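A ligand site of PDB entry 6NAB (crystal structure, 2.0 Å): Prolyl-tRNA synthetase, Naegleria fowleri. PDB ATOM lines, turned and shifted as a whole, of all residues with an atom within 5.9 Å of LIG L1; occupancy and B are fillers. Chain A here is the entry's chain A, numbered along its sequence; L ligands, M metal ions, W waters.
OG of Ser 272 is in hydrogen-bond range of N5 of LIG L1, at 2.7 Å. OE2 of Glu 152 sits at hydrogen-bond distance from N3 of LIG L1 (2.9 Å). The backbone carbonyl oxygen (O) of Gly 270 lies within hydrogen-bond range of an oxygen (O6) of LIG L1 (2.9 Å). OG1 of Thr 238 lies within hydrogen-bond range of O3 of LIG L1 (2.9 Å). N of Ser 162 sits at hydrogen-bond distance from N4 of LIG L1 (3.2 Å). A nitrogen (N3) of LIG L1 is in hydrogen-bond range of the backbone carbonyl oxygen (O) of Ser 162. NH1 of Arg 274 is in hydrogen-bond range of O7 of LIG L1 (3.2 Å). An oxygen (O2) of LIG L1 is in salt-bridge range of the guanidinium group (NH1) of Arg 150, 3.2 Å away. An oxygen (O7) of LIG L1 lies within hydrogen-bond range of the backbone carbonyl oxygen (O) of Gln 235, 3.5 Å away. NE2 of Gln 235 lies within hydrogen-bond range of O1 of LIG L1 (3.3 Å). NH2 of Arg 150 lies within salt-bridge range of O1 of LG2 L2 (2.9 Å). O2 of LG2 L2 sits at hydrogen-bond distance from NE2 of His 240, 2.8 Å away.
An oxygen (O2) of LG2 L2 sits close to an oxygen (O2) of LIG L1 (2.5 Å).
OG of Ser 272 sits at hydrogen-bond distance from N of Arg 274 (3.0 Å). O of Glu 152 sits at hydrogen-bond distance from NH2 of Arg 163. The backbone carbonyl oxygen (O) of Thr 238 lies within hydrogen-bond range of the backbone NH (N) of Gly 270. The side-chain hydroxyl (OG) of Ser 162 lies within hydrogen-bond range of the backbone carbonyl oxygen (O) of Glu 164 (2.6 Å). O of Gln 235 is in hydrogen-bond range of NH1 of Arg 274. The guanidinium group (NE) of Arg 274 sits at hydrogen-bond distance from the backbone carbonyl oxygen (O) of Ile 160. The backbone NH (N) of Gly 237 sits at hydrogen-bond distance from the side-chain amide oxygen (OE1) of Gln 235 (3.2 Å). ND1 of His 240 is in hydrogen-bond range of OG1 of Thr 220 (2.8 Å).
Phe 159 touches LIG L1 (O to C9, 3.6 Å). Ile 160 touches LIG L1. Arg 161 touches LIG L1 (CA to N4, 3.6 Å). Phe 165 touches LIG L1. Trp 167 touches LIG L1 (CE3 to O5, 3.7 Å). Gly 237 touches LIG L1. His 240 touches LIG L1 (CE1 to O3, 3.9 Å). CA of Leu 271 touches O6 of LIG L1, at 3.5 Å. Hydrophobic or aromatic side chains within 4 Å of LIG L1: Phe 165, Trp 167 and His 240. Of the 23 residues printed, 16 come within 4 Å of LIG L1. The nearest printed residue that does not touch LIG L1 is Phe 214 (4.1 Å).
Water W1 lies within hydrogen-bond range of the side-chain carboxylate of Glu 152 (2.6 Å), a nitrogen (N2) of LIG L1 (2.6 Å) and the guanidinium group of Arg 150 (3.4 Å). Water W2 lies within hydrogen-bond range of O of Gly 236, O6 of LIG L1 and N of Ser 272.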
ATOM      1  N   PHE A  95      24.182  26.720  30.787  1.00  0.00           N
ATOM      2  CA  PHE A  95      24.207  27.895  29.917  1.00  0.00           C
ATOM      3  C   PHE A  95      25.526  28.658  29.891  1.00  0.00           C
ATOM      4  O   PHE A  95      25.759  29.399  28.932  1.00  0.00           O
ATOM      5  CB  PHE A  95      23.076  28.872  30.308  1.00  0.00           C
ATOM      6  CG  PHE A  95      21.735  28.547  29.695  1.00  0.00           C
ATOM      7  CD1 PHE A  95      21.442  28.896  28.382  1.00  0.00           C
ATOM      8  CD2 PHE A  95      20.753  27.880  30.440  1.00  0.00           C
ATOM      9  CE1 PHE A  95      20.207  28.582  27.827  1.00  0.00           C
ATOM     10  CE2 PHE A  95      19.517  27.565  29.885  1.00  0.00           C
ATOM     11  CZ  PHE A  95      19.248  27.923  28.571  1.00  0.00           C
ATOM     12  N   ARG A 150      22.790  33.918  22.734  1.00  0.00           N
ATOM     13  CA  ARG A 150      23.432  32.673  23.103  1.00  0.00           C
ATOM     14  C   ARG A 150      24.651  32.505  22.215  1.00  0.00           C
ATOM     15  O   ARG A 150      24.521  32.402  20.992  1.00  0.00           O
ATOM     16  CB  ARG A 150      22.476  31.477  22.970  1.00  0.00           C
ATOM     17  CG  ARG A 150      21.373  31.511  24.033  1.00  0.00           C
ATOM     18  CD  ARG A 150      20.469  30.288  23.971  1.00  0.00           C
ATOM     19  NE  ARG A 150      19.303  30.513  24.826  1.00  0.00           N
ATOM     20  CZ  ARG A 150      18.344  29.622  25.087  1.00  0.00           C
ATOM     21  NH1 ARG A 150      18.394  28.393  24.572  1.00  0.00           N
ATOM     22  NH2 ARG A 150      17.340  29.985  25.866  1.00  0.00           N
ATOM     23  N   GLU A 152      26.474  30.648  20.605  1.00  0.00           N
ATOM     24  CA  GLU A 152      26.431  29.273  20.108  1.00  0.00           C
ATOM     25  C   GLU A 152      27.822  28.821  19.650  1.00  0.00           C
ATOM     26  O   GLU A 152      28.515  29.526  18.916  1.00  0.00           O
ATOM     27  CB  GLU A 152      25.436  29.141  18.947  1.00  0.00           C
ATOM     28  CG  GLU A 152      23.979  29.565  19.250  1.00  0.00           C
ATOM     29  CD  GLU A 152      23.181  28.469  19.980  1.00  0.00           C
ATOM     30  OE1 GLU A 152      23.593  27.290  19.944  1.00  0.00           O
ATOM     31  OE2 GLU A 152      22.127  28.790  20.582  1.00  0.00           O
ATOM     32  N   PHE A 159      18.014  31.987  11.036  1.00  0.00           N
ATOM     33  CA  PHE A 159      16.750  31.678  11.708  1.00  0.00           C
ATOM     34  C   PHE A 159      16.858  30.489  12.652  1.00  0.00           C
ATOM     35  O   PHE A 159      16.520  30.607  13.835  1.00  0.00           O
ATOM     36  CB  PHE A 159      15.615  31.405  10.709  1.00  0.00           C
ATOM     37  CG  PHE A 159      15.342  32.546   9.780  1.00  0.00           C
ATOM     38  CD1 PHE A 159      15.008  33.803  10.256  1.00  0.00           C
ATOM     39  CD2 PHE A 159      15.412  32.357   8.404  1.00  0.00           C
ATOM     40  CE1 PHE A 159      14.762  34.864   9.387  1.00  0.00           C
ATOM     41  CE2 PHE A 159      15.160  33.397   7.514  1.00  0.00           C
ATOM     42  CZ  PHE A 159      14.839  34.669   8.014  1.00  0.00           C
ATOM     43  N   ILE A 160      17.312  29.336  12.148  1.00  0.00           N
ATOM     44  CA  ILE A 160      17.310  28.108  12.946  1.00  0.00           C
ATOM     45  C   ILE A 160      18.190  28.269  14.175  1.00  0.00           C
ATOM     46  O   ILE A 160      17.811  27.873  15.283  1.00  0.00           O
ATOM     47  CB  ILE A 160      17.765  26.899  12.101  1.00  0.00           C
ATOM     48  CG1 ILE A 160      16.833  26.651  10.907  1.00  0.00           C
ATOM     49  CG2 ILE A 160      17.896  25.647  12.984  1.00  0.00           C
ATOM     50  CD1 ILE A 160      15.387  26.361  11.295  1.00  0.00           C
ATOM     51  N   ARG A 161      19.395  28.822  14.006  1.00  0.00           N
ATOM     52  CA  ARG A 161      20.372  28.871  15.096  1.00  0.00           C
ATOM     53  C   ARG A 161      21.212  30.142  14.939  1.00  0.00           C
ATOM     54  O   ARG A 161      22.276  30.136  14.317  1.00  0.00           O
ATOM     55  CB  ARG A 161      21.269  27.626  15.117  1.00  0.00           C
ATOM     56  CG  ARG A 161      22.264  27.612  16.283  1.00  0.00           C
ATOM     57  CD  ARG A 161      23.135  26.361  16.289  1.00  0.00           C
ATOM     58  NE  ARG A 161      22.316  25.134  16.350  1.00  0.00           N
ATOM     59  CZ  ARG A 161      21.728  24.700  17.464  1.00  0.00           C
ATOM     60  NH1 ARG A 161      21.854  25.373  18.599  1.00  0.00           N
ATOM     61  NH2 ARG A 161      21.003  23.583  17.424  1.00  0.00           N
ATOM     62  N   SER A 162      20.715  31.235  15.504  1.00  0.00           N
ATOM     63  CA  SER A 162      21.428  32.496  15.428  1.00  0.00           C
ATOM     64  C   SER A 162      21.971  32.847  16.806  1.00  0.00           C
ATOM     65  O   SER A 162      21.455  32.404  17.831  1.00  0.00           O
ATOM     66  CB  SER A 162      20.528  33.597  14.863  1.00  0.00           C
ATOM     67  OG  SER A 162      19.332  33.754  15.593  1.00  0.00           O
ATOM     68  N   ARG A 163      23.058  33.617  16.820  1.00  0.00           N
ATOM     69  CA  ARG A 163      23.633  33.982  18.113  1.00  0.00           C
ATOM     70  C   ARG A 163      22.815  35.050  18.825  1.00  0.00           C
ATOM     71  O   ARG A 163      22.773  35.057  20.056  1.00  0.00           O
ATOM     72  CB  ARG A 163      25.068  34.455  17.923  1.00  0.00           C
ATOM     73  CG  ARG A 163      26.016  33.286  17.790  1.00  0.00           C
ATOM     74  CD  ARG A 163      27.442  33.745  18.000  1.00  0.00           C
ATOM     75  NE  ARG A 163      28.370  32.613  18.013  1.00  0.00           N
ATOM     76  CZ  ARG A 163      29.689  32.755  17.877  1.00  0.00           C
ATOM     77  NH1 ARG A 163      30.206  33.963  17.713  1.00  0.00           N
ATOM     78  NH2 ARG A 163      30.478  31.692  17.908  1.00  0.00           N
ATOM     79  N   GLU A 164      22.181  35.947  18.089  1.00  0.00           N
ATOM     80  CA  GLU A 164      21.073  36.731  18.628  1.00  0.00           C
ATOM     81  C   GLU A 164      19.805  36.238  17.959  1.00  0.00           C
ATOM     82  O   GLU A 164      19.768  36.029  16.741  1.00  0.00           O
ATOM     83  CB  GLU A 164      21.258  38.247  18.402  1.00  0.00           C
ATOM     84  CG  GLU A 164      20.046  39.064  18.896  1.00  0.00           C
ATOM     85  CD  GLU A 164      20.103  40.566  18.520  1.00  0.00           C
ATOM     86  OE1 GLU A 164      20.840  40.950  17.572  1.00  0.00           O
ATOM     87  OE2 GLU A 164      19.373  41.342  19.165  1.00  0.00           O
ATOM     88  N   PHE A 165      18.768  35.992  18.759  1.00  0.00           N
ATOM     89  CA  PHE A 165      17.493  35.647  18.174  1.00  0.00           C
ATOM     90  C   PHE A 165      16.400  36.360  18.959  1.00  0.00           C
ATOM     91  O   PHE A 165      16.637  36.935  20.028  1.00  0.00           O
ATOM     92  CB  PHE A 165      17.265  34.109  18.113  1.00  0.00           C
ATOM     93  CG  PHE A 165      17.323  33.402  19.446  1.00  0.00           C
ATOM     94  CD1 PHE A 165      16.159  33.163  20.176  1.00  0.00           C
ATOM     95  CD2 PHE A 165      18.532  32.912  19.941  1.00  0.00           C
ATOM     96  CE1 PHE A 165      16.210  32.476  21.401  1.00  0.00           C
ATOM     97  CE2 PHE A 165      18.599  32.240  21.160  1.00  0.00           C
ATOM     98  CZ  PHE A 165      17.430  32.015  21.893  1.00  0.00           C
ATOM     99  N   TRP A 167      12.322  36.206  20.450  1.00  0.00           N
ATOM    100  CA  TRP A 167      11.366  35.218  20.913  1.00  0.00           C
ATOM    101  C   TRP A 167      10.299  35.907  21.744  1.00  0.00           C
ATOM    102  O   TRP A 167      10.343  37.120  21.965  1.00  0.00           O
ATOM    103  CB  TRP A 167      12.081  34.094  21.695  1.00  0.00           C
ATOM    104  CG  TRP A 167      12.597  34.419  23.108  1.00  0.00           C
ATOM    105  CD1 TRP A 167      12.589  35.625  23.766  1.00  0.00           C
ATOM    106  CD2 TRP A 167      13.215  33.479  24.011  1.00  0.00           C
ATOM    107  NE1 TRP A 167      13.152  35.487  25.024  1.00  0.00           N
ATOM    108  CE2 TRP A 167      13.545  34.193  25.202  1.00  0.00           C
ATOM    109  CE3 TRP A 167      13.519  32.116  23.935  1.00  0.00           C
ATOM    110  CZ2 TRP A 167      14.171  33.568  26.292  1.00  0.00           C
ATOM    111  CZ3 TRP A 167      14.140  31.495  25.039  1.00  0.00           C
ATOM    112  CH2 TRP A 167      14.453  32.233  26.194  1.00  0.00           C
ATOM    113  N   PHE A 214      15.203  20.891  29.700  1.00  0.00           N
ATOM    114  CA  PHE A 214      15.747  22.163  30.169  1.00  0.00           C
ATOM    115  C   PHE A 214      16.377  21.999  31.549  1.00  0.00           C
ATOM    116  O   PHE A 214      15.838  21.306  32.412  1.00  0.00           O
ATOM    117  CB  PHE A 214      14.610  23.200  30.205  1.00  0.00           C
ATOM    118  CG  PHE A 214      15.053  24.632  30.437  1.00  0.00           C
ATOM    119  CD1 PHE A 214      15.822  25.304  29.492  1.00  0.00           C
ATOM    120  CD2 PHE A 214      14.621  25.330  31.554  1.00  0.00           C
ATOM    121  CE1 PHE A 214      16.200  26.626  29.697  1.00  0.00           C
ATOM    122  CE2 PHE A 214      14.997  26.672  31.768  1.00  0.00           C
ATOM    123  CZ  PHE A 214      15.786  27.316  30.845  1.00  0.00           C
ATOM    124  N   THR A 220      10.173  18.758  30.110  1.00  0.00           N
ATOM    125  CA  THR A 220      10.092  19.668  28.975  1.00  0.00           C
ATOM    126  C   THR A 220       9.229  19.024  27.916  1.00  0.00           C
ATOM    127  O   THR A 220       9.439  17.845  27.577  1.00  0.00           O
ATOM    128  CB  THR A 220      11.489  19.971  28.412  1.00  0.00           C
ATOM    129  OG1 THR A 220      12.240  20.760  29.356  1.00  0.00           O
ATOM    130  CG2 THR A 220      11.387  20.724  27.076  1.00  0.00           C
ATOM    131  N   GLN A 235      13.663  21.168  16.713  1.00  0.00           N
ATOM    132  CA  GLN A 235      12.878  21.483  17.897  1.00  0.00           C
ATOM    133  C   GLN A 235      12.243  22.859  17.713  1.00  0.00           C
ATOM    134  O   GLN A 235      12.937  23.885  17.695  1.00  0.00           O
ATOM    135  CB  GLN A 235      13.772  21.438  19.142  1.00  0.00           C
ATOM    136  CG  GLN A 235      13.047  21.780  20.440  1.00  0.00           C
ATOM    137  CD  GLN A 235      13.415  23.158  20.975  1.00  0.00           C
ATOM    138  OE1 GLN A 235      12.712  24.135  20.711  1.00  0.00           O
ATOM    139  NE2 GLN A 235      14.528  23.244  21.704  1.00  0.00           N
ATOM    140  N   GLY A 236      10.917  22.905  17.539  1.00  0.00           N
ATOM    141  CA  GLY A 236      10.261  24.110  17.081  1.00  0.00           C
ATOM    142  C   GLY A 236       9.791  25.081  18.148  1.00  0.00           C
ATOM    143  O   GLY A 236       9.380  26.196  17.808  1.00  0.00           O
ATOM    144  N   GLY A 237       9.847  24.700  19.424  1.00  0.00           N
ATOM    145  CA  GLY A 237       9.309  25.488  20.511  1.00  0.00           C
ATOM    146  C   GLY A 237       9.146  24.601  21.732  1.00  0.00           C
ATOM    147  O   GLY A 237       8.891  23.404  21.578  1.00  0.00           O
ATOM    148  N   THR A 238       9.308  25.149  22.942  1.00  0.00           N
ATOM    149  CA  THR A 238       9.313  24.300  24.128  1.00  0.00           C
ATOM    150  C   THR A 238       8.492  24.925  25.239  1.00  0.00           C
ATOM    151  O   THR A 238       8.431  26.147  25.382  1.00  0.00           O
ATOM    152  CB  THR A 238      10.737  24.045  24.650  1.00  0.00           C
ATOM    153  OG1 THR A 238      11.483  25.258  24.597  1.00  0.00           O
ATOM    154  CG2 THR A 238      11.440  22.968  23.823  1.00  0.00           C
ATOM    155  N   HIS A 240       8.096  24.239  29.339  1.00  0.00           N
ATOM    156  CA  HIS A 240       8.705  23.544  30.479  1.00  0.00           C
ATOM    157  C   HIS A 240       7.858  23.621  31.738  1.00  0.00           C
ATOM    158  O   HIS A 240       7.352  24.696  32.089  1.00  0.00           O
ATOM    159  CB  HIS A 240      10.086  24.125  30.828  1.00  0.00           C
ATOM    160  CG  HIS A 240      10.965  24.394  29.658  1.00  0.00           C
ATOM    161  ND1 HIS A 240      11.497  23.383  28.877  1.00  0.00           N
ATOM    162  CD2 HIS A 240      11.473  25.552  29.180  1.00  0.00           C
ATOM    163  CE1 HIS A 240      12.263  23.928  27.947  1.00  0.00           C
ATOM    164  NE2 HIS A 240      12.276  25.234  28.111  1.00  0.00           N
ATOM    165  N   GLY A 270       8.882  29.133  25.554  1.00  0.00           N
ATOM    166  CA  GLY A 270       9.462  30.028  24.572  1.00  0.00           C
ATOM    167  C   GLY A 270       9.333  29.576  23.120  1.00  0.00           C
ATOM    168  O   GLY A 270       9.472  28.381  22.806  1.00  0.00           O
ATOM    169  N   LEU A 271       9.043  30.535  22.252  1.00  0.00           N
ATOM    170  CA  LEU A 271       8.927  30.349  20.801  1.00  0.00           C
ATOM    171  C   LEU A 271       9.740  31.464  20.148  1.00  0.00           C
ATOM    172  O   LEU A 271       9.616  32.625  20.538  1.00  0.00           O
ATOM    173  CB  LEU A 271       7.468  30.445  20.351  1.00  0.00           C
ATOM    174  CG  LEU A 271       7.167  30.164  18.881  1.00  0.00           C
ATOM    175  CD1 LEU A 271       7.177  28.658  18.650  1.00  0.00           C
ATOM    176  CD2 LEU A 271       5.826  30.758  18.498  1.00  0.00           C
ATOM    177  N   SER A 272      10.565  31.106  19.159  1.00  0.00           N
ATOM    178  CA  SER A 272      11.514  32.058  18.602  1.00  0.00           C
ATOM    179  C   SER A 272      11.371  32.182  17.088  1.00  0.00           C
ATOM    180  O   SER A 272      10.599  31.459  16.436  1.00  0.00           O
ATOM    181  CB  SER A 272      12.947  31.639  18.936  1.00  0.00           C
ATOM    182  OG  SER A 272      13.381  30.635  18.033  1.00  0.00           O
ATOM    183  N   THR A 273      12.197  33.063  16.513  1.00  0.00           N
ATOM    184  CA  THR A 273      12.303  33.234  15.062  1.00  0.00           C
ATOM    185  C   THR A 273      12.857  32.009  14.348  1.00  0.00           C
ATOM    186  O   THR A 273      12.904  31.998  13.105  1.00  0.00           O
ATOM    187  CB  THR A 273      13.164  34.477  14.749  1.00  0.00           C
ATOM    188  OG1 THR A 273      14.295  34.547  15.650  1.00  0.00           O
ATOM    189  CG2 THR A 273      12.325  35.740  14.883  1.00  0.00           C
ATOM    190  N   ARG A 274      13.220  30.960  15.079  1.00  0.00           N
ATOM    191  CA  ARG A 274      13.458  29.671  14.446  1.00  0.00           C
ATOM    192  C   ARG A 274      12.251  29.237  13.607  1.00  0.00           C
ATOM    193  O   ARG A 274      12.414  28.604  12.556  1.00  0.00           O
ATOM    194  CB  ARG A 274      13.791  28.629  15.519  1.00  0.00           C
ATOM    195  CG  ARG A 274      13.818  27.167  15.045  1.00  0.00           C
ATOM    196  CD  ARG A 274      14.338  26.252  16.161  1.00  0.00           C
ATOM    197  NE  ARG A 274      15.744  26.474  16.476  1.00  0.00           N
ATOM    198  CZ  ARG A 274      16.390  25.883  17.481  1.00  0.00           C
ATOM    199  NH1 ARG A 274      15.738  25.039  18.286  1.00  0.00           N
ATOM    200  NH2 ARG A 274      17.674  26.139  17.682  1.00  0.00           N
HETATM  201  P1  LIG L   1      15.571  25.672  24.324  1.00  0.00           P
HETATM  202  O1  LIG L   1      16.674  24.951  23.560  1.00  0.00           O
HETATM  203  O2  LIG L   1      16.020  26.539  25.613  1.00  0.00           O
HETATM  204  O3  LIG L   1      14.374  24.779  24.724  1.00  0.00           O
HETATM  205  O4  LIG L   1      14.929  26.685  23.295  1.00  0.00           O
HETATM  206  C1  LIG L   1      13.942  27.632  23.715  1.00  0.00           C
HETATM  207  C2  LIG L   1      13.347  28.354  22.542  1.00  0.00           C
HETATM  208  O5  LIG L   1      14.387  29.125  21.877  1.00  0.00           O
HETATM  209  C3  LIG L   1      12.740  27.461  21.466  1.00  0.00           C
HETATM  210  O6  LIG L   1      11.646  28.146  20.864  1.00  0.00           O
HETATM  211  C4  LIG L   1      13.870  27.310  20.456  1.00  0.00           C
HETATM  212  O7  LIG L   1      13.434  27.014  19.150  1.00  0.00           O
HETATM  213  C5  LIG L   1      14.548  28.684  20.540  1.00  0.00           C
HETATM  214  N1  LIG L   1      15.983  28.710  20.251  1.00  0.00           N
HETATM  215  C6  LIG L   1      16.986  28.184  21.028  1.00  0.00           C
HETATM  216  N2  LIG L   1      18.201  28.466  20.605  1.00  0.00           N
HETATM  217  C7  LIG L   1      17.979  29.226  19.464  1.00  0.00           C
HETATM  218  C8  LIG L   1      18.858  29.858  18.568  1.00  0.00           C
HETATM  219  N3  LIG L   1      20.191  29.856  18.696  1.00  0.00           N
HETATM  220  N4  LIG L   1      18.316  30.548  17.529  1.00  0.00           N
HETATM  221  C9  LIG L   1      16.982  30.604  17.434  1.00  0.00           C
HETATM  222  N5  LIG L   1      16.054  30.047  18.226  1.00  0.00           N
HETATM  223  C10 LIG L   1      16.621  29.375  19.222  1.00  0.00           C
HETATM  224  N1  LG2 L   2      13.323  29.878  29.176  1.00  0.00           N
HETATM  225  C1  LG2 L   2      13.029  28.560  28.600  1.00  0.00           C
HETATM  226  C2  LG2 L   2      14.086  28.204  27.561  1.00  0.00           C
HETATM  227  O1  LG2 L   2      15.023  29.000  27.346  1.00  0.00           O
HETATM  228  C3  LG2 L   2      11.645  28.742  27.948  1.00  0.00           C
HETATM  229  C4  LG2 L   2      11.582  30.238  27.646  1.00  0.00           C
HETATM  230  C5  LG2 L   2      12.309  30.889  28.801  1.00  0.00           C
HETATM  231  O2  LG2 L   2      14.027  27.143  26.936  1.00  0.00           O
HETATM  232 MG    MG M   1      20.763  25.574  22.967  1.00  0.00          MG
HETATM  233  O   HOH W   1      20.281  27.496  21.874  1.00  0.00           O
HETATM  234  O   HOH W   2      10.991  28.374  18.127  1.00  0.00           O
HETATM  235  O   HOH W   3      15.078  22.556  26.263  1.00  0.00           O
